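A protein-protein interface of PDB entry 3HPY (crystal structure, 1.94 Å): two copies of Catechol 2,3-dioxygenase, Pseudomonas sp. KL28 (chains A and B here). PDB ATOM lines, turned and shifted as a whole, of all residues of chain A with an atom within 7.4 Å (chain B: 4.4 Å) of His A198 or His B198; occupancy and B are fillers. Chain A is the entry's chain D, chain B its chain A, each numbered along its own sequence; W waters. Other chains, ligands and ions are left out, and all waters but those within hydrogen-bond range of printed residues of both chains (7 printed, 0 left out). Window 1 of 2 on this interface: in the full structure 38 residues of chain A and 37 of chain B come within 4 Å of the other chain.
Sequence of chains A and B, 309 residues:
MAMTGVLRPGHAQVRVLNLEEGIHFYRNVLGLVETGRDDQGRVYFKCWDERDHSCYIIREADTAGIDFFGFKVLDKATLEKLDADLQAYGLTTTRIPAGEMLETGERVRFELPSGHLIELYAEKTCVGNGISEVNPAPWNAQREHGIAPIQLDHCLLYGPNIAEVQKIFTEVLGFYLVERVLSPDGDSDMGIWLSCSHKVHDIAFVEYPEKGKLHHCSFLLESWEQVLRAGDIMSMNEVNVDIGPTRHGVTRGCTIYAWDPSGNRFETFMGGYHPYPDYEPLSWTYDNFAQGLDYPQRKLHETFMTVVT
NE2 of His B198 sits at hydrogen-bond distance from NE2 of His A198 (3.1 Å). The backbone carbonyl oxygen (O) of Ala A2 sits close to the side-chain sulfur (SD) of Met B3, at 3.7 Å. SD of Met A3 lies close to SD of Met B3 (3.6 Å).
The backbone carbonyl oxygen (O) of Ser B197 sits at hydrogen-bond distance from the side-chain hydroxyl (OH) of Tyr B176 (2.9 Å). The side-chain hydroxyl of Tyr B176 sits at hydrogen-bond distance from the backbone NH of Tyr B276, 3.2 Å away. The backbone carbonyl oxygen (O) of Leu A7 is in hydrogen-bond range of the side-chain sulfur (SG) of Cys A196 (3.4 Å). The backbone NH of Tyr A276 sits at hydrogen-bond distance from the side-chain hydroxyl of Tyr A176 (3.2 Å). OG of Ser A195 lies within hydrogen-bond range of O of Ser A197 (3.0 Å). The backbone carbonyl oxygen (O) of Lys A199 is in hydrogen-bond range of the side-chain hydroxyl (OG) of Ser A195, 2.8 Å away.
Among the printed residues, merely in contact across the chains: Met A3 with Ser B197 (3.9 Å), Leu A7 with Tyr B276 (3.7 Å), Arg A8 with Tyr B276 (3.1 Å), Cys A196 with Met B3 (3.8 Å), Ser A197 with Met B3 (3.9 Å), Ser A197 with His B198 (3.4 Å), His A198 with Ser B197 (3.4 Å), His A198 with Lys B199 (3.4 Å), Lys A199 with His B198 (3.2 Å), Tyr A276 with Lys B199 (3.8 Å) and Pro A277 with Met B3 (3.4 Å).
His A198 touches just these residues of chain B: Ser B197 (3.4 Å), His B198 (3.1 Å) and Lys B199 (3.4 Å). Of the printed residues of chain B, Ser A197 touches Met B3 (3.9 Å) and His B198 (3.4 Å). Printed residues of chain B within 4 Å of Pro A277: Met B3. Ser A195 touches none of the printed residues of chain B. The nearest residue of chain B that does not touch His A198 is Met B3 (4.1 Å). The nearest printed residue of chain A that does not touch Tyr B276 is Met A3 (4.1 Å).
Along chain B the printed residues that touch a printed residue of chain A span positions 3 to 276. Of the 20 printed residues of chain A, 10 touch a printed residue of chain B. Hydrophobic or aromatic side chains of chain A within 4 Å of the printed part of chain B: Met A3, His A198, Tyr A276 and Pro A277. Along chain A the printed residues that touch a printed residue of chain B span positions 2 to 277. Among the printed residues, 14 pairs touch across the chains.
Met A3 touches Ser B197, and with the chains exchanged Ser A197 touches Met B3. Ser A197 touches His B198, and with the chains exchanged His A198 touches Ser B197. His A198 touches Lys B199, and with the chains exchanged Lys A199 touches His B198. Tyr A276 touches Lys B199, but with the chains exchanged Lys A199 does not touch Tyr B276 (4.2 Å). Of the 14 pairs that touch across the chains among the printed residues, 8 have their exchanged pair printed and touching as well.
Water W4 lies within hydrogen-bond range of the side-chain hydroxyl (OH) of Tyr B276 (2.7 Å), the side-chain carboxylate (OD1) of Asp A202 (2.8 Å), the backbone carbonyl oxygen (O) of Leu A7 (2.8 Å) and the side-chain hydroxyl (OG) of Ser A197 (3.1 Å). Water W1 lies within hydrogen-bond range of the backbone NH of Met A3 (2.8 Å) and the backbone carbonyl oxygen of Ser B197 (3.1 Å). Water W5 lies within hydrogen-bond range of the backbone NH (N) of Met B3 (2.8 Å) and the backbone carbonyl oxygen (O) of Ser A197 (3.0 Å). Water W3 bridges the side-chain hydroxyl of Tyr A276 (2.8 Å) and the side-chain hydroxyl of Ser B197 (3.3 Å). Water W6 lies within hydrogen-bond range of NZ of Lys A199 (2.9 Å), OH of Tyr B276 (3.1 Å) and NE2 of Gln A151 (3.2 Å). Water W2 bridges the side-chain amide oxygen of Gln A151 (3.0 Å) and the side-chain hydroxyl of Tyr B276 (3.1 Å).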
ATOM      1  N   ALA A   2       9.171 -17.540  25.008  1.00  0.00           N
ATOM      2  CA  ALA A   2       8.827 -16.394  24.118  1.00  0.00           C
ATOM      3  C   ALA A   2       9.623 -16.434  22.822  1.00  0.00           C
ATOM      4  O   ALA A   2      10.787 -16.833  22.816  1.00  0.00           O
ATOM      5  CB  ALA A   2       9.120 -15.085  24.832  1.00  0.00           C
ATOM      6  N   MET A   3       8.993 -16.024  21.726  1.00  0.00           N
ATOM      7  CA  MET A   3       9.683 -15.947  20.446  1.00  0.00           C
ATOM      8  C   MET A   3      10.285 -14.546  20.419  1.00  0.00           C
ATOM      9  O   MET A   3       9.578 -13.557  20.628  1.00  0.00           O
ATOM     10  CB  MET A   3       8.713 -16.092  19.272  1.00  0.00           C
ATOM     11  CG  MET A   3       8.386 -17.441  18.873  1.00  0.00           C
ATOM     12  SD  MET A   3       9.888 -18.184  18.245  1.00  0.00           S
ATOM     13  CE  MET A   3      10.169 -17.641  16.669  1.00  0.00           C
ATOM     14  N   LEU A   7      12.078 -14.147  14.045  1.00  0.00           N
ATOM     15  CA  LEU A   7      10.845 -14.892  14.257  1.00  0.00           C
ATOM     16  C   LEU A   7      10.579 -15.983  13.225  1.00  0.00           C
ATOM     17  O   LEU A   7      10.429 -17.147  13.574  1.00  0.00           O
ATOM     18  CB  LEU A   7       9.647 -13.937  14.283  1.00  0.00           C
ATOM     19  CG  LEU A   7       9.714 -12.796  15.296  1.00  0.00           C
ATOM     20  CD1 LEU A   7       8.459 -11.948  15.209  1.00  0.00           C
ATOM     21  CD2 LEU A   7       9.880 -13.381  16.694  1.00  0.00           C
ATOM     22  N   ARG A   8      10.519 -15.616  11.952  1.00  0.00           N
ATOM     23  CA  ARG A   8      10.214 -16.621  10.942  1.00  0.00           C
ATOM     24  C   ARG A   8      10.500 -16.164   9.516  1.00  0.00           C
ATOM     25  O   ARG A   8      10.779 -14.987   9.279  1.00  0.00           O
ATOM     26  CB  ARG A   8       8.733 -17.000  11.040  1.00  0.00           C
ATOM     27  CG  ARG A   8       7.765 -15.981  10.402  1.00  0.00           C
ATOM     28  CD  ARG A   8       7.323 -14.895  11.349  1.00  0.00           C
ATOM     29  NE  ARG A   8       6.395 -13.932  10.743  1.00  0.00           N
ATOM     30  CZ  ARG A   8       5.603 -13.146  11.462  1.00  0.00           C
ATOM     31  NH1 ARG A   8       5.643 -13.248  12.779  1.00  0.00           N
ATOM     32  NH2 ARG A   8       4.817 -12.239  10.890  1.00  0.00           N
ATOM     33  N   GLN A 151       1.379 -21.109   4.909  1.00  0.00           N
ATOM     34  CA  GLN A 151       2.497 -20.196   5.164  1.00  0.00           C
ATOM     35  C   GLN A 151       3.711 -20.588   4.360  1.00  0.00           C
ATOM     36  O   GLN A 151       3.786 -21.697   3.832  1.00  0.00           O
ATOM     37  CB  GLN A 151       2.906 -20.208   6.654  1.00  0.00           C
ATOM     38  CG  GLN A 151       3.354 -21.580   7.218  1.00  0.00           C
ATOM     39  CD  GLN A 151       4.009 -21.503   8.611  1.00  0.00           C
ATOM     40  OE1 GLN A 151       3.631 -20.687   9.454  1.00  0.00           O
ATOM     41  NE2 GLN A 151       4.981 -22.378   8.853  1.00  0.00           N
ATOM     42  N   TYR A 176      19.251 -22.866  15.562  1.00  0.00           N
ATOM     43  CA  TYR A 176      19.877 -24.056  16.124  1.00  0.00           C
ATOM     44  C   TYR A 176      19.724 -25.228  15.167  1.00  0.00           C
ATOM     45  O   TYR A 176      18.785 -25.272  14.369  1.00  0.00           O
ATOM     46  CB  TYR A 176      19.326 -24.376  17.530  1.00  0.00           C
ATOM     47  CG  TYR A 176      17.870 -24.762  17.624  1.00  0.00           C
ATOM     48  CD1 TYR A 176      17.485 -26.103  17.677  1.00  0.00           C
ATOM     49  CD2 TYR A 176      16.872 -23.790  17.676  1.00  0.00           C
ATOM     50  CE1 TYR A 176      16.143 -26.462  17.782  1.00  0.00           C
ATOM     51  CE2 TYR A 176      15.533 -24.138  17.772  1.00  0.00           C
ATOM     52  CZ  TYR A 176      15.177 -25.476  17.824  1.00  0.00           C
ATOM     53  OH  TYR A 176      13.850 -25.830  17.896  1.00  0.00           O
ATOM     54  N   VAL A 178      18.613 -28.592  13.930  1.00  0.00           N
ATOM     55  CA  VAL A 178      17.559 -29.561  14.252  1.00  0.00           C
ATOM     56  C   VAL A 178      17.951 -30.936  13.727  1.00  0.00           C
ATOM     57  O   VAL A 178      17.882 -31.934  14.446  1.00  0.00           O
ATOM     58  CB  VAL A 178      16.194 -29.139  13.644  1.00  0.00           C
ATOM     59  CG1 VAL A 178      15.162 -30.253  13.816  1.00  0.00           C
ATOM     60  CG2 VAL A 178      15.701 -27.885  14.324  1.00  0.00           C
ATOM     61  N   SER A 195      16.550 -24.186  12.702  1.00  0.00           N
ATOM     62  CA  SER A 195      15.332 -23.608  13.251  1.00  0.00           C
ATOM     63  C   SER A 195      15.600 -22.370  14.128  1.00  0.00           C
ATOM     64  O   SER A 195      16.595 -22.317  14.863  1.00  0.00           O
ATOM     65  CB  SER A 195      14.599 -24.684  14.064  1.00  0.00           C
ATOM     66  OG  SER A 195      13.455 -24.172  14.726  1.00  0.00           O
ATOM     67  N   CYS A 196      14.718 -21.377  14.034  1.00  0.00           N
ATOM     68  CA  CYS A 196      14.825 -20.168  14.853  1.00  0.00           C
ATOM     69  C   CYS A 196      13.554 -20.105  15.703  1.00  0.00           C
ATOM     70  O   CYS A 196      13.162 -19.050  16.207  1.00  0.00           O
ATOM     71  CB  CYS A 196      14.936 -18.918  13.974  1.00  0.00           C
ATOM     72  SG  CYS A 196      13.512 -18.523  12.935  1.00  0.00           S
ATOM     73  N   SER A 197      12.931 -21.266  15.876  1.00  0.00           N
ATOM     74  CA  SER A 197      11.674 -21.362  16.618  1.00  0.00           C
ATOM     75  C   SER A 197      11.495 -22.797  17.085  1.00  0.00           C
ATOM     76  O   SER A 197      12.481 -23.453  17.423  1.00  0.00           O
ATOM     77  CB  SER A 197      10.532 -20.963  15.681  1.00  0.00           C
ATOM     78  OG  SER A 197      10.503 -21.790  14.524  1.00  0.00           O
ATOM     79  N   HIS A 198      10.256 -23.289  17.162  1.00  0.00           N
ATOM     80  CA  HIS A 198      10.100 -24.688  17.536  1.00  0.00           C
ATOM     81  C   HIS A 198       9.630 -25.489  16.327  1.00  0.00           C
ATOM     82  O   HIS A 198       9.118 -26.586  16.451  1.00  0.00           O
ATOM     83  CB  HIS A 198       9.187 -24.910  18.761  1.00  0.00           C
ATOM     84  CG  HIS A 198       7.791 -24.425  18.594  1.00  0.00           C
ATOM     85  ND1 HIS A 198       7.352 -23.242  19.146  1.00  0.00           N
ATOM     86  CD2 HIS A 198       6.717 -24.985  17.992  1.00  0.00           C
ATOM     87  CE1 HIS A 198       6.066 -23.089  18.891  1.00  0.00           C
ATOM     88  NE2 HIS A 198       5.654 -24.135  18.199  1.00  0.00           N
ATOM     89  N   LYS A 199       9.838 -24.928  15.142  1.00  0.00           N
ATOM     90  CA  LYS A 199       9.497 -25.637  13.915  1.00  0.00           C
ATOM     91  C   LYS A 199      10.668 -26.573  13.588  1.00  0.00           C
ATOM     92  O   LYS A 199      11.805 -26.316  13.990  1.00  0.00           O
ATOM     93  CB  LYS A 199       9.289 -24.653  12.769  1.00  0.00           C
ATOM     94  CG  LYS A 199       8.040 -23.798  12.912  1.00  0.00           C
ATOM     95  CD  LYS A 199       7.615 -23.283  11.557  1.00  0.00           C
ATOM     96  CE  LYS A 199       8.703 -22.462  10.922  1.00  0.00           C
ATOM     97  NZ  LYS A 199       8.464 -22.222   9.480  1.00  0.00           N
ATOM     98  N   VAL A 200      10.407 -27.663  12.878  1.00  0.00           N
ATOM     99  CA  VAL A 200      11.494 -28.580  12.543  1.00  0.00           C
ATOM    100  C   VAL A 200      12.594 -27.832  11.780  1.00  0.00           C
ATOM    101  O   VAL A 200      13.763 -28.196  11.849  1.00  0.00           O
ATOM    102  CB  VAL A 200      11.004 -29.791  11.708  1.00  0.00           C
ATOM    103  CG1 VAL A 200      10.288 -29.318  10.452  1.00  0.00           C
ATOM    104  CG2 VAL A 200      12.199 -30.677  11.348  1.00  0.00           C
ATOM    105  N   HIS A 201      12.221 -26.782  11.053  1.00  0.00           N
ATOM    106  CA  HIS A 201      13.214 -25.989  10.336  1.00  0.00           C
ATOM    107  C   HIS A 201      12.588 -24.786   9.651  1.00  0.00           C
ATOM    108  O   HIS A 201      11.454 -24.852   9.164  1.00  0.00           O
ATOM    109  CB  HIS A 201      13.981 -26.848   9.313  1.00  0.00           C
ATOM    110  CG  HIS A 201      13.136 -27.371   8.189  1.00  0.00           C
ATOM    111  ND1 HIS A 201      11.866 -27.869   8.381  1.00  0.00           N
ATOM    112  CD2 HIS A 201      13.396 -27.505   6.866  1.00  0.00           C
ATOM    113  CE1 HIS A 201      11.380 -28.288   7.226  1.00  0.00           C
ATOM    114  NE2 HIS A 201      12.289 -28.079   6.291  1.00  0.00           N
ATOM    115  N   ASP A 202      13.326 -23.679   9.657  1.00  0.00           N
ATOM    116  CA  ASP A 202      12.896 -22.441   9.034  1.00  0.00           C
ATOM    117  C   ASP A 202      13.746 -22.213   7.794  1.00  0.00           C
ATOM    118  O   ASP A 202      13.433 -21.359   6.963  1.00  0.00           O
ATOM    119  CB  ASP A 202      13.073 -21.266   9.994  1.00  0.00           C
ATOM    120  CG  ASP A 202      12.076 -21.291  11.130  1.00  0.00           C
ATOM    121  OD1 ASP A 202      10.937 -20.808  10.936  1.00  0.00           O
ATOM    122  OD2 ASP A 202      12.431 -21.804  12.212  1.00  0.00           O
ATOM    123  N   TYR A 273       8.064 -33.016  13.673  1.00  0.00           N
ATOM    124  CA  TYR A 273       7.998 -32.952  15.119  1.00  0.00           C
ATOM    125  C   TYR A 273       8.172 -31.517  15.602  1.00  0.00           C
ATOM    126  O   TYR A 273       8.190 -30.596  14.797  1.00  0.00           O
ATOM    127  CB  TYR A 273       9.049 -33.873  15.734  1.00  0.00           C
ATOM    128  CG  TYR A 273      10.429 -33.698  15.163  1.00  0.00           C
ATOM    129  CD1 TYR A 273      11.357 -32.851  15.770  1.00  0.00           C
ATOM    130  CD2 TYR A 273      10.826 -34.411  14.035  1.00  0.00           C
ATOM    131  CE1 TYR A 273      12.659 -32.723  15.272  1.00  0.00           C
ATOM    132  CE2 TYR A 273      12.127 -34.291  13.524  1.00  0.00           C
ATOM    133  CZ  TYR A 273      13.037 -33.447  14.152  1.00  0.00           C
ATOM    134  OH  TYR A 273      14.325 -33.347  13.669  1.00  0.00           O
ATOM    135  N   HIS A 274       8.307 -31.336  16.916  1.00  0.00           N
ATOM    136  CA  HIS A 274       8.416 -30.005  17.517  1.00  0.00           C
ATOM    137  C   HIS A 274       9.696 -29.771  18.304  1.00  0.00           C
ATOM    138  O   HIS A 274       9.668 -29.776  19.534  1.00  0.00           O
ATOM    139  CB  HIS A 274       7.257 -29.757  18.471  1.00  0.00           C
ATOM    140  CG  HIS A 274       5.918 -30.185  17.849  1.00  0.00           C
ATOM    141  ND1 HIS A 274       5.237 -29.404  16.939  1.00  0.00           N
ATOM    142  CD2 HIS A 274       5.203 -31.327  17.973  1.00  0.00           C
ATOM    143  CE1 HIS A 274       4.161 -30.049  16.529  1.00  0.00           C
ATOM    144  NE2 HIS A 274       4.117 -31.219  17.140  1.00  0.00           N
ATOM    145  N   PRO A 275      10.823 -29.567  17.605  1.00  0.00           N
ATOM    146  CA  PRO A 275      12.090 -29.341  18.304  1.00  0.00           C
ATOM    147  C   PRO A 275      12.105 -28.033  19.103  1.00  0.00           C
ATOM    148  O   PRO A 275      11.366 -27.100  18.802  1.00  0.00           O
ATOM    149  CB  PRO A 275      13.105 -29.289  17.174  1.00  0.00           C
ATOM    150  CG  PRO A 275      12.332 -28.827  15.968  1.00  0.00           C
ATOM    151  CD  PRO A 275      10.899 -29.248  16.157  1.00  0.00           C
ATOM    152  N   TYR A 276      12.959 -27.982  20.118  1.00  0.00           N
ATOM    153  CA  TYR A 276      13.104 -26.823  20.946  1.00  0.00           C
ATOM    154  C   TYR A 276      14.618 -26.564  21.086  1.00  0.00           C
ATOM    155  O   TYR A 276      15.398 -27.499  20.945  1.00  0.00           O
ATOM    156  CB  TYR A 276      12.465 -27.019  22.324  1.00  0.00           C
ATOM    157  CG  TYR A 276      10.956 -26.761  22.333  1.00  0.00           C
ATOM    158  CD1 TYR A 276      10.442 -25.529  22.731  1.00  0.00           C
ATOM    159  CD2 TYR A 276      10.076 -27.748  21.930  1.00  0.00           C
ATOM    160  CE1 TYR A 276       9.090 -25.281  22.723  1.00  0.00           C
ATOM    161  CE2 TYR A 276       8.717 -27.504  21.897  1.00  0.00           C
ATOM    162  CZ  TYR A 276       8.225 -26.275  22.291  1.00  0.00           C
ATOM    163  OH  TYR A 276       6.865 -26.043  22.233  1.00  0.00           O
ATOM    164  N   PRO A 277      15.039 -25.318  21.392  1.00  0.00           N
ATOM    165  CA  PRO A 277      16.453 -24.934  21.508  1.00  0.00           C
ATOM    166  C   PRO A 277      17.295 -25.828  22.430  1.00  0.00           C
ATOM    167  O   PRO A 277      18.523 -25.860  22.308  1.00  0.00           O
ATOM    168  CB  PRO A 277      16.394 -23.513  22.025  1.00  0.00           C
ATOM    169  CG  PRO A 277      15.114 -22.997  21.490  1.00  0.00           C
ATOM    170  CD  PRO A 277      14.157 -24.158  21.563  1.00  0.00           C
ATOM    171  N   MET B   3      13.700 -19.067  20.000  1.00  0.00           N
ATOM    172  CA  MET B   3      12.899 -19.398  21.186  1.00  0.00           C
ATOM    173  C   MET B   3      13.720 -19.093  22.421  1.00  0.00           C
ATOM    174  O   MET B   3      14.850 -19.563  22.529  1.00  0.00           O
ATOM    175  CB  MET B   3      12.460 -20.877  21.135  1.00  0.00           C
ATOM    176  CG  MET B   3      11.072 -21.116  20.564  1.00  0.00           C
ATOM    177  SD  MET B   3       9.824 -20.062  21.340  1.00  0.00           S
ATOM    178  CE  MET B   3       9.881 -20.660  23.026  1.00  0.00           C
ATOM    179  N   TYR B 176       2.102 -13.784  25.334  1.00  0.00           N
ATOM    180  CA  TYR B 176       1.267 -12.830  24.621  1.00  0.00           C
ATOM    181  C   TYR B 176      -0.115 -13.420  24.360  1.00  0.00           C
ATOM    182  O   TYR B 176      -0.274 -14.638  24.215  1.00  0.00           O
ATOM    183  CB  TYR B 176       1.939 -12.394  23.313  1.00  0.00           C
ATOM    184  CG  TYR B 176       2.029 -13.460  22.249  1.00  0.00           C
ATOM    185  CD1 TYR B 176       1.113 -13.504  21.196  1.00  0.00           C
ATOM    186  CD2 TYR B 176       3.058 -14.398  22.265  1.00  0.00           C
ATOM    187  CE1 TYR B 176       1.230 -14.453  20.181  1.00  0.00           C
ATOM    188  CE2 TYR B 176       3.181 -15.350  21.265  1.00  0.00           C
ATOM    189  CZ  TYR B 176       2.266 -15.372  20.224  1.00  0.00           C
ATOM    190  OH  TYR B 176       2.395 -16.304  19.221  1.00  0.00           O
ATOM    191  N   SER B 195       0.241 -17.502  24.787  1.00  0.00           N
ATOM    192  CA  SER B 195       1.318 -18.257  24.153  1.00  0.00           C
ATOM    193  C   SER B 195       2.702 -17.701  24.503  1.00  0.00           C
ATOM    194  O   SER B 195       2.858 -16.499  24.699  1.00  0.00           O
ATOM    195  CB  SER B 195       1.125 -18.235  22.626  1.00  0.00           C
ATOM    196  OG  SER B 195       2.238 -18.781  21.934  1.00  0.00           O
ATOM    197  N   SER B 197       5.281 -18.905  22.592  1.00  0.00           N
ATOM    198  CA  SER B 197       5.933 -19.472  21.410  1.00  0.00           C
ATOM    199  C   SER B 197       5.122 -19.100  20.165  1.00  0.00           C
ATOM    200  O   SER B 197       4.619 -17.988  20.059  1.00  0.00           O
ATOM    201  CB  SER B 197       5.954 -20.995  21.555  1.00  0.00           C
ATOM    202  OG  SER B 197       4.633 -21.481  21.771  1.00  0.00           O
ATOM    203  N   HIS B 198       5.020 -20.002  19.191  1.00  0.00           N
ATOM    204  CA  HIS B 198       4.152 -19.687  18.066  1.00  0.00           C
ATOM    205  C   HIS B 198       2.954 -20.637  18.025  1.00  0.00           C
ATOM    206  O   HIS B 198       2.289 -20.784  16.995  1.00  0.00           O
ATOM    207  CB  HIS B 198       4.886 -19.598  16.686  1.00  0.00           C
ATOM    208  CG  HIS B 198       5.614 -20.838  16.248  1.00  0.00           C
ATOM    209  ND1 HIS B 198       6.968 -20.995  16.391  1.00  0.00           N
ATOM    210  CD2 HIS B 198       5.188 -21.966  15.636  1.00  0.00           C
ATOM    211  CE1 HIS B 198       7.350 -22.165  15.914  1.00  0.00           C
ATOM    212  NE2 HIS B 198       6.283 -22.779  15.448  1.00  0.00           N
ATOM    213  N   LYS B 199       2.679 -21.270  19.169  1.00  0.00           N
ATOM    214  CA  LYS B 199       1.531 -22.163  19.297  1.00  0.00           C
ATOM    215  C   LYS B 199       0.300 -21.323  19.650  1.00  0.00           C
ATOM    216  O   LYS B 199       0.441 -20.256  20.244  1.00  0.00           O
ATOM    217  CB  LYS B 199       1.760 -23.213  20.391  1.00  0.00           C
ATOM    218  CG  LYS B 199       2.704 -24.328  19.962  1.00  0.00           C
ATOM    219  CD  LYS B 199       2.665 -25.494  20.930  1.00  0.00           C
ATOM    220  CE  LYS B 199       3.182 -25.091  22.266  1.00  0.00           C
ATOM    221  NZ  LYS B 199       2.541 -25.845  23.397  1.00  0.00           N
ATOM    222  N   VAL B 200      -0.890 -21.790  19.258  1.00  0.00           N
ATOM    223  CA  VAL B 200      -2.135 -21.076  19.553  1.00  0.00           C
ATOM    224  C   VAL B 200      -2.220 -20.740  21.032  1.00  0.00           C
ATOM    225  O   VAL B 200      -2.683 -19.663  21.387  1.00  0.00           O
ATOM    226  CB  VAL B 200      -3.399 -21.878  19.167  1.00  0.00           C
ATOM    227  CG1 VAL B 200      -3.737 -21.636  17.717  1.00  0.00           C
ATOM    228  CG2 VAL B 200      -3.180 -23.357  19.434  1.00  0.00           C
ATOM    229  N   HIS B 274      -0.993 -20.557  13.411  1.00  0.00           N
ATOM    230  CA  HIS B 274       0.340 -20.300  13.949  1.00  0.00           C
ATOM    231  C   HIS B 274       0.637 -18.860  14.252  1.00  0.00           C
ATOM    232  O   HIS B 274       1.311 -18.187  13.477  1.00  0.00           O
ATOM    233  CB  HIS B 274       1.380 -20.797  12.958  1.00  0.00           C
ATOM    234  CG  HIS B 274       1.071 -22.145  12.400  1.00  0.00           C
ATOM    235  ND1 HIS B 274       1.467 -23.313  13.015  1.00  0.00           N
ATOM    236  CD2 HIS B 274       0.360 -22.513  11.307  1.00  0.00           C
ATOM    237  CE1 HIS B 274       1.016 -24.344  12.322  1.00  0.00           C
ATOM    238  NE2 HIS B 274       0.342 -23.886  11.282  1.00  0.00           N
ATOM    239  N   PRO B 275       0.165 -18.373  15.401  1.00  0.00           N
ATOM    240  CA  PRO B 275       0.369 -16.987  15.835  1.00  0.00           C
ATOM    241  C   PRO B 275       1.836 -16.691  16.187  1.00  0.00           C
ATOM    242  O   PRO B 275       2.620 -17.598  16.499  1.00  0.00           O
ATOM    243  CB  PRO B 275      -0.529 -16.888  17.060  1.00  0.00           C
ATOM    244  CG  PRO B 275      -0.313 -18.254  17.692  1.00  0.00           C
ATOM    245  CD  PRO B 275      -0.428 -19.184  16.483  1.00  0.00           C
ATOM    246  N   TYR B 276       2.198 -15.417  16.115  1.00  0.00           N
ATOM    247  CA  TYR B 276       3.542 -14.967  16.467  1.00  0.00           C
ATOM    248  C   TYR B 276       3.367 -13.744  17.361  1.00  0.00           C
ATOM    249  O   TYR B 276       2.352 -13.054  17.288  1.00  0.00           O
ATOM    250  CB  TYR B 276       4.373 -14.632  15.213  1.00  0.00           C
ATOM    251  CG  TYR B 276       4.997 -15.860  14.565  1.00  0.00           C
ATOM    252  CD1 TYR B 276       6.265 -16.316  14.937  1.00  0.00           C
ATOM    253  CD2 TYR B 276       4.297 -16.586  13.606  1.00  0.00           C
ATOM    254  CE1 TYR B 276       6.821 -17.491  14.355  1.00  0.00           C
ATOM    255  CE2 TYR B 276       4.833 -17.743  13.021  1.00  0.00           C
ATOM    256  CZ  TYR B 276       6.083 -18.192  13.394  1.00  0.00           C
ATOM    257  OH  TYR B 276       6.568 -19.343  12.811  1.00  0.00           O
HETATM  258  O   HOH W   1       6.222 -15.867  21.632  1.00  0.00           O
HETATM  259  O   HOH W   2       4.401 -21.498  12.230  1.00  0.00           O
HETATM  260  O   HOH W   3       5.833 -23.839  23.699  1.00  0.00           O
HETATM  261  O   HOH W   4       9.233 -19.566  12.782  1.00  0.00           O
HETATM  262  O   HOH W   5      14.350 -21.552  18.898  1.00  0.00           O
HETATM  263  O   HOH W   6       6.832 -19.894   9.822  1.00  0.00           O
HETATM  264  O   HOH W   7       4.909 -27.709  23.566  1.00  0.00           O
